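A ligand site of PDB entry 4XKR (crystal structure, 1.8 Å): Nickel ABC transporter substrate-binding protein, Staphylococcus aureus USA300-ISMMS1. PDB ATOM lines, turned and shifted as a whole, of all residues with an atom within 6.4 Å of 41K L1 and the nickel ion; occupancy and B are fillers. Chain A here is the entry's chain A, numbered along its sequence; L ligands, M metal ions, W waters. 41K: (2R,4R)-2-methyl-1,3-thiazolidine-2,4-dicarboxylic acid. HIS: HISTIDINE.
An oxygen (OXT) of 41K L1 sits close to the guanidinium group (NH2) of Arg 325, at 3.8 Å.
OH of Tyr 381 lies close to SAK of 41K L1, at 3.8 Å.
The guanidinium group (NE) of Arg 325 lies within salt-bridge range of an oxygen (OXT) of HIS L2 (2.9 Å).
The backbone NH (N) of Gly 372 sits at hydrogen-bond distance from an oxygen (OAD) of 41K L1 (2.8 Å).
The backbone carbonyl oxygen (O) of Ser 370 sits close to a nitrogen (N) of HIS L2, 3.1 Å away.
OE2 of Glu 355 sits close to N of HIS L2, 3.8 Å away.
OH of Tyr 369 sits close to N of HIS L2, at 3.1 Å.
NH2 of Arg 234 lies within salt-bridge range of OAD of 41K L1 (3.8 Å).
The guanidinium group (NH1) of Arg 234 sits close to an oxygen (O) of HIS L2.
OH of Tyr 322 sits at hydrogen-bond distance from OXT of HIS L2, 2.7 Å away.
N of Ser 370 lies within hydrogen-bond range of OH of Tyr 322 (3.4 Å).
The guanidinium group (NH1) of Arg 234 lies within hydrogen-bond range of the side-chain hydroxyl (OG) of Ser 370 (3.0 Å).
The backbone carbonyl oxygen (O) of Ser 370 lies close to an oxygen (OAA) of 41K L1 (3.4 Å).
Residues that only touch 41K L1: Ile 393 (3.5 Å), Asp 28 (3.6 Å), Phe 371 (3.6 Å), Phe 134 (3.6 Å) and Tyr 369 (3.7 Å).
Of the 20 residues printed, 10 come within 4 Å of 41K L1.
The nearest printed residue that does not touch 41K L1 is Glu 355 (4.8 Å).
No residue comes within 4 Å of the nickel ion.
The nearest printed residue that does not touch the nickel ion is Ser 370 (4.1 Å).
The nickel ion is bound by OAA of 41K L1, N of HIS L2, O of HIS L2, ND1 of HIS L2, N of 41K L1 and OXT of 41K L1.
The nickel ion has six donor atoms within binding distance.
Water W2 lies within hydrogen-bond range of O of 41K L1, N of Asp 28 and OG1 of Thr 27.
Water W3 lies within hydrogen-bond range of OAD of 41K L1 (2.6 Å), O of Gly 372 (2.7 Å) and OH of Tyr 381 (2.7 Å).
Water W1 lies within hydrogen-bond range of O of 41K L1 and OD2 of Asp 28.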
ATOM      1  N   LEU A  17     -22.633  23.195  -9.615  1.00  0.00           N
ATOM      2  CA  LEU A  17     -21.976  24.477  -9.275  1.00  0.00           C
ATOM      3  C   LEU A  17     -22.910  25.677  -9.412  1.00  0.00           C
ATOM      4  O   LEU A  17     -22.730  26.545 -10.279  1.00  0.00           O
ATOM      5  CB  LEU A  17     -20.696  24.682 -10.117  1.00  0.00           C
ATOM      6  CG  LEU A  17     -19.714  23.499 -10.040  1.00  0.00           C
ATOM      7  CD1 LEU A  17     -18.394  23.805 -10.816  1.00  0.00           C
ATOM      8  CD2 LEU A  17     -19.436  23.089  -8.591  1.00  0.00           C
ATOM      9  N   GLU A  26     -19.462  37.372 -13.878  1.00  0.00           N
ATOM     10  CA  GLU A  26     -19.439  36.621 -12.609  1.00  0.00           C
ATOM     11  C   GLU A  26     -19.358  35.105 -12.810  1.00  0.00           C
ATOM     12  O   GLU A  26     -19.025  34.363 -11.887  1.00  0.00           O
ATOM     13  CB  GLU A  26     -20.680  36.925 -11.751  1.00  0.00           C
ATOM     14  CG  GLU A  26     -20.771  38.360 -11.254  1.00  0.00           C
ATOM     15  CD  GLU A  26     -19.764  38.700 -10.151  1.00  0.00           C
ATOM     16  OE1 GLU A  26     -18.995  37.824  -9.702  1.00  0.00           O
ATOM     17  OE2 GLU A  26     -19.747  39.879  -9.736  1.00  0.00           O
ATOM     18  N   THR A  27     -19.698  34.648 -14.007  1.00  0.00           N
ATOM     19  CA  THR A  27     -19.772  33.210 -14.273  1.00  0.00           C
ATOM     20  C   THR A  27     -19.824  32.938 -15.771  1.00  0.00           C
ATOM     21  O   THR A  27     -20.304  33.765 -16.529  1.00  0.00           O
ATOM     22  CB  THR A  27     -21.016  32.583 -13.608  1.00  0.00           C
ATOM     23  OG1 THR A  27     -21.205  31.242 -14.093  1.00  0.00           O
ATOM     24  CG2 THR A  27     -22.238  33.411 -13.916  1.00  0.00           C
ATOM     25  N   ASP A  28     -19.302  31.777 -16.182  1.00  0.00           N
ATOM     26  CA  ASP A  28     -19.355  31.400 -17.592  1.00  0.00           C
ATOM     27  C   ASP A  28     -20.683  30.757 -17.981  1.00  0.00           C
ATOM     28  O   ASP A  28     -20.876  30.380 -19.127  1.00  0.00           O
ATOM     29  CB  ASP A  28     -18.178  30.489 -17.923  1.00  0.00           C
ATOM     30  CG  ASP A  28     -18.343  29.048 -17.433  1.00  0.00           C
ATOM     31  OD1 ASP A  28     -19.280  28.743 -16.671  1.00  0.00           O
ATOM     32  OD2 ASP A  28     -17.485  28.222 -17.804  1.00  0.00           O
ATOM     33  N   LEU A  98     -11.355  39.468 -12.029  1.00  0.00           N
ATOM     34  CA  LEU A  98     -10.902  38.503 -13.027  1.00  0.00           C
ATOM     35  C   LEU A  98     -10.757  39.199 -14.363  1.00  0.00           C
ATOM     36  O   LEU A  98      -9.697  39.117 -15.009  1.00  0.00           O
ATOM     37  CB  LEU A  98     -11.863  37.312 -13.142  1.00  0.00           C
ATOM     38  CG  LEU A  98     -11.414  36.072 -13.948  1.00  0.00           C
ATOM     39  CD1 LEU A  98     -12.213  34.845 -13.506  1.00  0.00           C
ATOM     40  CD2 LEU A  98     -11.560  36.260 -15.477  1.00  0.00           C
ATOM     41  N   PHE A 134     -15.991  35.223 -19.380  1.00  0.00           N
ATOM     42  CA  PHE A 134     -16.266  36.295 -18.407  1.00  0.00           C
ATOM     43  C   PHE A 134     -16.289  37.668 -19.106  1.00  0.00           C
ATOM     44  O   PHE A 134     -16.741  38.662 -18.525  1.00  0.00           O
ATOM     45  CB  PHE A 134     -15.216  36.296 -17.286  1.00  0.00           C
ATOM     46  CG  PHE A 134     -15.455  35.265 -16.211  1.00  0.00           C
ATOM     47  CD1 PHE A 134     -15.193  33.921 -16.454  1.00  0.00           C
ATOM     48  CD2 PHE A 134     -15.932  35.644 -14.959  1.00  0.00           C
ATOM     49  CE1 PHE A 134     -15.423  32.966 -15.461  1.00  0.00           C
ATOM     50  CE2 PHE A 134     -16.153  34.691 -13.968  1.00  0.00           C
ATOM     51  CZ  PHE A 134     -15.903  33.353 -14.213  1.00  0.00           C
ATOM     52  N   ARG A 234      -9.117  20.352 -17.921  1.00  0.00           N
ATOM     53  CA  ARG A 234      -9.500  20.538 -16.519  1.00  0.00           C
ATOM     54  C   ARG A 234      -8.669  19.603 -15.637  1.00  0.00           C
ATOM     55  O   ARG A 234      -8.454  18.431 -15.971  1.00  0.00           O
ATOM     56  CB  ARG A 234     -10.985  20.266 -16.320  1.00  0.00           C
ATOM     57  CG  ARG A 234     -11.467  20.509 -14.866  1.00  0.00           C
ATOM     58  CD  ARG A 234     -12.927  20.894 -14.824  1.00  0.00           C
ATOM     59  NE  ARG A 234     -13.181  22.283 -15.220  1.00  0.00           N
ATOM     60  CZ  ARG A 234     -13.065  23.340 -14.417  1.00  0.00           C
ATOM     61  NH1 ARG A 234     -12.676  23.201 -13.149  1.00  0.00           N
ATOM     62  NH2 ARG A 234     -13.347  24.561 -14.896  1.00  0.00           N
ATOM     63  N   TYR A 322     -16.660  19.346  -2.155  1.00  0.00           N
ATOM     64  CA  TYR A 322     -17.983  19.678  -2.684  1.00  0.00           C
ATOM     65  C   TYR A 322     -18.370  18.629  -3.704  1.00  0.00           C
ATOM     66  O   TYR A 322     -17.501  17.933  -4.249  1.00  0.00           O
ATOM     67  CB  TYR A 322     -18.010  21.087  -3.300  1.00  0.00           C
ATOM     68  CG  TYR A 322     -16.967  21.362  -4.375  1.00  0.00           C
ATOM     69  CD1 TYR A 322     -15.615  21.504  -4.044  1.00  0.00           C
ATOM     70  CD2 TYR A 322     -17.335  21.483  -5.726  1.00  0.00           C
ATOM     71  CE1 TYR A 322     -14.653  21.760  -5.023  1.00  0.00           C
ATOM     72  CE2 TYR A 322     -16.376  21.752  -6.701  1.00  0.00           C
ATOM     73  CZ  TYR A 322     -15.050  21.890  -6.343  1.00  0.00           C
ATOM     74  OH  TYR A 322     -14.088  22.156  -7.305  1.00  0.00           O
ATOM     75  N   ARG A 325     -18.015  18.401  -8.811  1.00  0.00           N
ATOM     76  CA  ARG A 325     -17.152  17.489  -9.552  1.00  0.00           C
ATOM     77  C   ARG A 325     -17.179  16.184  -8.752  1.00  0.00           C
ATOM     78  O   ARG A 325     -16.649  16.115  -7.650  1.00  0.00           O
ATOM     79  CB  ARG A 325     -15.714  18.026  -9.666  1.00  0.00           C
ATOM     80  CG  ARG A 325     -15.557  19.475 -10.078  1.00  0.00           C
ATOM     81  CD  ARG A 325     -15.987  19.726 -11.541  1.00  0.00           C
ATOM     82  NE  ARG A 325     -15.809  21.138 -11.885  1.00  0.00           N
ATOM     83  CZ  ARG A 325     -16.182  21.690 -13.042  1.00  0.00           C
ATOM     84  NH1 ARG A 325     -16.741  20.944 -13.984  1.00  0.00           N
ATOM     85  NH2 ARG A 325     -15.966  22.994 -13.262  1.00  0.00           N
ATOM     86  N   GLU A 355     -17.342  28.300  -3.519  1.00  0.00           N
ATOM     87  CA  GLU A 355     -16.663  29.596  -3.553  1.00  0.00           C
ATOM     88  C   GLU A 355     -17.127  30.493  -2.419  1.00  0.00           C
ATOM     89  O   GLU A 355     -16.325  31.238  -1.861  1.00  0.00           O
ATOM     90  CB  GLU A 355     -16.875  30.301  -4.892  1.00  0.00           C
ATOM     91  CG  GLU A 355     -16.271  29.570  -6.074  1.00  0.00           C
ATOM     92  CD  GLU A 355     -14.790  29.232  -5.888  1.00  0.00           C
ATOM     93  OE1 GLU A 355     -14.130  29.695  -4.929  1.00  0.00           O
ATOM     94  OE2 GLU A 355     -14.272  28.500  -6.738  1.00  0.00           O
ATOM     95  N   TYR A 369     -10.294  20.755  -5.194  1.00  0.00           N
ATOM     96  CA  TYR A 369     -10.619  21.813  -6.123  1.00  0.00           C
ATOM     97  C   TYR A 369     -10.452  21.332  -7.548  1.00  0.00           C
ATOM     98  O   TYR A 369      -9.954  20.237  -7.775  1.00  0.00           O
ATOM     99  CB  TYR A 369      -9.759  23.040  -5.828  1.00  0.00           C
ATOM    100  CG  TYR A 369     -10.403  24.352  -6.231  1.00  0.00           C
ATOM    101  CD1 TYR A 369     -11.523  24.851  -5.544  1.00  0.00           C
ATOM    102  CD2 TYR A 369      -9.913  25.066  -7.309  1.00  0.00           C
ATOM    103  CE1 TYR A 369     -12.104  26.081  -5.936  1.00  0.00           C
ATOM    104  CE2 TYR A 369     -10.500  26.286  -7.694  1.00  0.00           C
ATOM    105  CZ  TYR A 369     -11.579  26.781  -7.018  1.00  0.00           C
ATOM    106  OH  TYR A 369     -12.121  27.981  -7.463  1.00  0.00           O
ATOM    107  N   SER A 370     -10.880  22.146  -8.499  1.00  0.00           N
ATOM    108  CA  SER A 370     -10.774  21.804  -9.901  1.00  0.00           C
ATOM    109  C   SER A 370     -10.593  23.088 -10.683  1.00  0.00           C
ATOM    110  O   SER A 370     -11.355  24.038 -10.485  1.00  0.00           O
ATOM    111  CB  SER A 370     -12.021  21.060 -10.384  1.00  0.00           C
ATOM    112  OG  SER A 370     -11.882  20.665 -11.731  1.00  0.00           O
ATOM    113  N   PHE A 371      -9.580  23.129 -11.544  1.00  0.00           N
ATOM    114  CA  PHE A 371      -9.252  24.320 -12.321  1.00  0.00           C
ATOM    115  C   PHE A 371      -9.393  24.031 -13.817  1.00  0.00           C
ATOM    116  O   PHE A 371      -8.929  22.991 -14.277  1.00  0.00           O
ATOM    117  CB  PHE A 371      -7.780  24.758 -12.094  1.00  0.00           C
ATOM    118  CG  PHE A 371      -7.536  25.694 -10.916  1.00  0.00           C
ATOM    119  CD1 PHE A 371      -8.292  26.834 -10.729  1.00  0.00           C
ATOM    120  CD2 PHE A 371      -6.461  25.468 -10.067  1.00  0.00           C
ATOM    121  CE1 PHE A 371      -8.014  27.706  -9.678  1.00  0.00           C
ATOM    122  CE2 PHE A 371      -6.181  26.326  -9.020  1.00  0.00           C
ATOM    123  CZ  PHE A 371      -6.957  27.456  -8.838  1.00  0.00           C
ATOM    124  N   GLY A 372      -9.963  24.969 -14.581  1.00  0.00           N
ATOM    125  CA  GLY A 372      -9.757  24.931 -16.020  1.00  0.00           C
ATOM    126  C   GLY A 372      -8.451  25.648 -16.286  1.00  0.00           C
ATOM    127  O   GLY A 372      -8.427  26.873 -16.286  1.00  0.00           O
ATOM    128  N   THR A 373      -7.373  24.906 -16.482  1.00  0.00           N
ATOM    129  CA  THR A 373      -6.043  25.521 -16.404  1.00  0.00           C
ATOM    130  C   THR A 373      -5.509  26.109 -17.699  1.00  0.00           C
ATOM    131  O   THR A 373      -4.532  26.856 -17.666  1.00  0.00           O
ATOM    132  CB  THR A 373      -4.971  24.537 -15.865  1.00  0.00           C
ATOM    133  OG1 THR A 373      -4.821  23.434 -16.756  1.00  0.00           O
ATOM    134  CG2 THR A 373      -5.392  24.029 -14.482  1.00  0.00           C
ATOM    135  N   TYR A 381      -2.930  32.901 -18.625  1.00  0.00           N
ATOM    136  CA  TYR A 381      -4.179  33.130 -17.909  1.00  0.00           C
ATOM    137  C   TYR A 381      -4.129  32.475 -16.536  1.00  0.00           C
ATOM    138  O   TYR A 381      -4.384  33.107 -15.517  1.00  0.00           O
ATOM    139  CB  TYR A 381      -5.364  32.575 -18.721  1.00  0.00           C
ATOM    140  CG  TYR A 381      -6.593  32.245 -17.874  1.00  0.00           C
ATOM    141  CD1 TYR A 381      -7.468  33.232 -17.448  1.00  0.00           C
ATOM    142  CD2 TYR A 381      -6.865  30.925 -17.525  1.00  0.00           C
ATOM    143  CE1 TYR A 381      -8.583  32.930 -16.682  1.00  0.00           C
ATOM    144  CE2 TYR A 381      -7.974  30.597 -16.766  1.00  0.00           C
ATOM    145  CZ  TYR A 381      -8.833  31.601 -16.340  1.00  0.00           C
ATOM    146  OH  TYR A 381      -9.942  31.267 -15.589  1.00  0.00           O
ATOM    147  N   ALA A 392      -7.704  36.301  -9.557  1.00  0.00           N
ATOM    148  CA  ALA A 392      -9.120  36.074  -9.201  1.00  0.00           C
ATOM    149  C   ALA A 392      -9.461  34.624  -8.828  1.00  0.00           C
ATOM    150  O   ALA A 392     -10.478  34.388  -8.188  1.00  0.00           O
ATOM    151  CB  ALA A 392     -10.004  36.510 -10.338  1.00  0.00           C
ATOM    152  N   ILE A 393      -8.638  33.663  -9.221  1.00  0.00           N
ATOM    153  CA  ILE A 393      -8.928  32.283  -8.881  1.00  0.00           C
ATOM    154  C   ILE A 393      -7.904  31.706  -7.897  1.00  0.00           C
ATOM    155  O   ILE A 393      -7.905  30.504  -7.630  1.00  0.00           O
ATOM    156  CB  ILE A 393      -9.034  31.420 -10.178  1.00  0.00           C
ATOM    157  CG1 ILE A 393      -7.671  31.190 -10.840  1.00  0.00           C
ATOM    158  CG2 ILE A 393     -10.029  32.091 -11.162  1.00  0.00           C
ATOM    159  CD1 ILE A 393      -7.748  30.422 -12.197  1.00  0.00           C
ATOM    160  N   LYS A 395      -7.531  31.132  -4.709  1.00  0.00           N
ATOM    161  CA  LYS A 395      -8.345  31.089  -3.501  1.00  0.00           C
ATOM    162  C   LYS A 395      -7.498  30.915  -2.230  1.00  0.00           C
ATOM    163  O   LYS A 395      -7.892  31.414  -1.171  1.00  0.00           O
ATOM    164  CB  LYS A 395      -9.409  29.972  -3.575  1.00  0.00           C
ATOM    165  CG  LYS A 395     -10.256  29.945  -4.876  1.00  0.00           C
ATOM    166  CD  LYS A 395     -10.766  31.328  -5.258  1.00  0.00           C
ATOM    167  CE  LYS A 395     -11.765  31.258  -6.421  1.00  0.00           C
ATOM    168  NZ  LYS A 395     -12.318  32.612  -6.725  1.00  0.00           N
ATOM    169  N   ILE A 462     -16.189  24.738 -21.562  1.00  0.00           N
ATOM    170  CA  ILE A 462     -16.967  25.947 -21.288  1.00  0.00           C
ATOM    171  C   ILE A 462     -18.278  25.919 -22.101  1.00  0.00           C
ATOM    172  O   ILE A 462     -19.366  26.095 -21.546  1.00  0.00           O
ATOM    173  CB  ILE A 462     -16.166  27.221 -21.652  1.00  0.00           C
ATOM    174  CG1 ILE A 462     -14.987  27.387 -20.696  1.00  0.00           C
ATOM    175  CG2 ILE A 462     -17.071  28.466 -21.630  1.00  0.00           C
ATOM    176  CD1 ILE A 462     -14.008  28.470 -21.137  1.00  0.00           C
HETATM  177  OAA 41K L   1     -12.889  26.233 -12.511  1.00  0.00           O
HETATM  178  CAE 41K L   1     -12.133  27.231 -12.682  1.00  0.00           C
HETATM  179  OAD 41K L   1     -11.101  27.236 -13.369  1.00  0.00           O
HETATM  180  CAF 41K L   1     -12.589  28.563 -12.084  1.00  0.00           C
HETATM  181  CAB 41K L   1     -11.642  28.959 -10.955  1.00  0.00           C
HETATM  182  N   41K L   1     -13.949  28.540 -11.502  1.00  0.00           N
HETATM  183  SAK 41K L   1     -12.638  29.795 -13.389  1.00  0.00           S
HETATM  184  CB  41K L   1     -14.339  30.257 -13.138  1.00  0.00           C
HETATM  185  CA  41K L   1     -14.963  28.995 -12.471  1.00  0.00           C
HETATM  186  C   41K L   1     -15.491  27.992 -13.515  1.00  0.00           C
HETATM  187  O   41K L   1     -15.990  28.516 -14.544  1.00  0.00           O
HETATM  188  OXT 41K L   1     -15.430  26.766 -13.223  1.00  0.00           O
HETATM  189  N   HIS L   2     -13.429  26.127  -9.599  1.00  0.00           N
HETATM  190  CA  HIS L   2     -14.198  25.038  -8.985  1.00  0.00           C
HETATM  191  C   HIS L   2     -14.717  24.079 -10.043  1.00  0.00           C
HETATM  192  O   HIS L   2     -14.766  24.437 -11.223  1.00  0.00           O
HETATM  193  CB  HIS L   2     -15.352  25.585  -8.138  1.00  0.00           C
HETATM  194  CG  HIS L   2     -16.395  26.350  -8.919  1.00  0.00           C
HETATM  195  ND1 HIS L   2     -16.186  26.826 -10.193  1.00  0.00           N
HETATM  196  CD2 HIS L   2     -17.650  26.721  -8.571  1.00  0.00           C
HETATM  197  CE1 HIS L   2     -17.288  27.460 -10.610  1.00  0.00           C
HETATM  198  NE2 HIS L   2     -18.174  27.407  -9.640  1.00  0.00           N
HETATM  199  OXT HIS L   2     -15.064  22.929  -9.713  1.00  0.00           O
HETATM  200 NI    NI M   1     -14.478  26.485 -11.339  1.00  0.00          NI
HETATM  201  O   HOH W   1     -14.939  28.341 -16.963  1.00  0.00           O
HETATM  202  O   HOH W   2     -17.927  30.202 -13.943  1.00  0.00           O
HETATM  203  O   HOH W   3     -10.393  28.584 -15.524  1.00  0.00           O
HETATM  204  O   HOH W   4     -17.254  25.137 -14.808  1.00  0.00           O
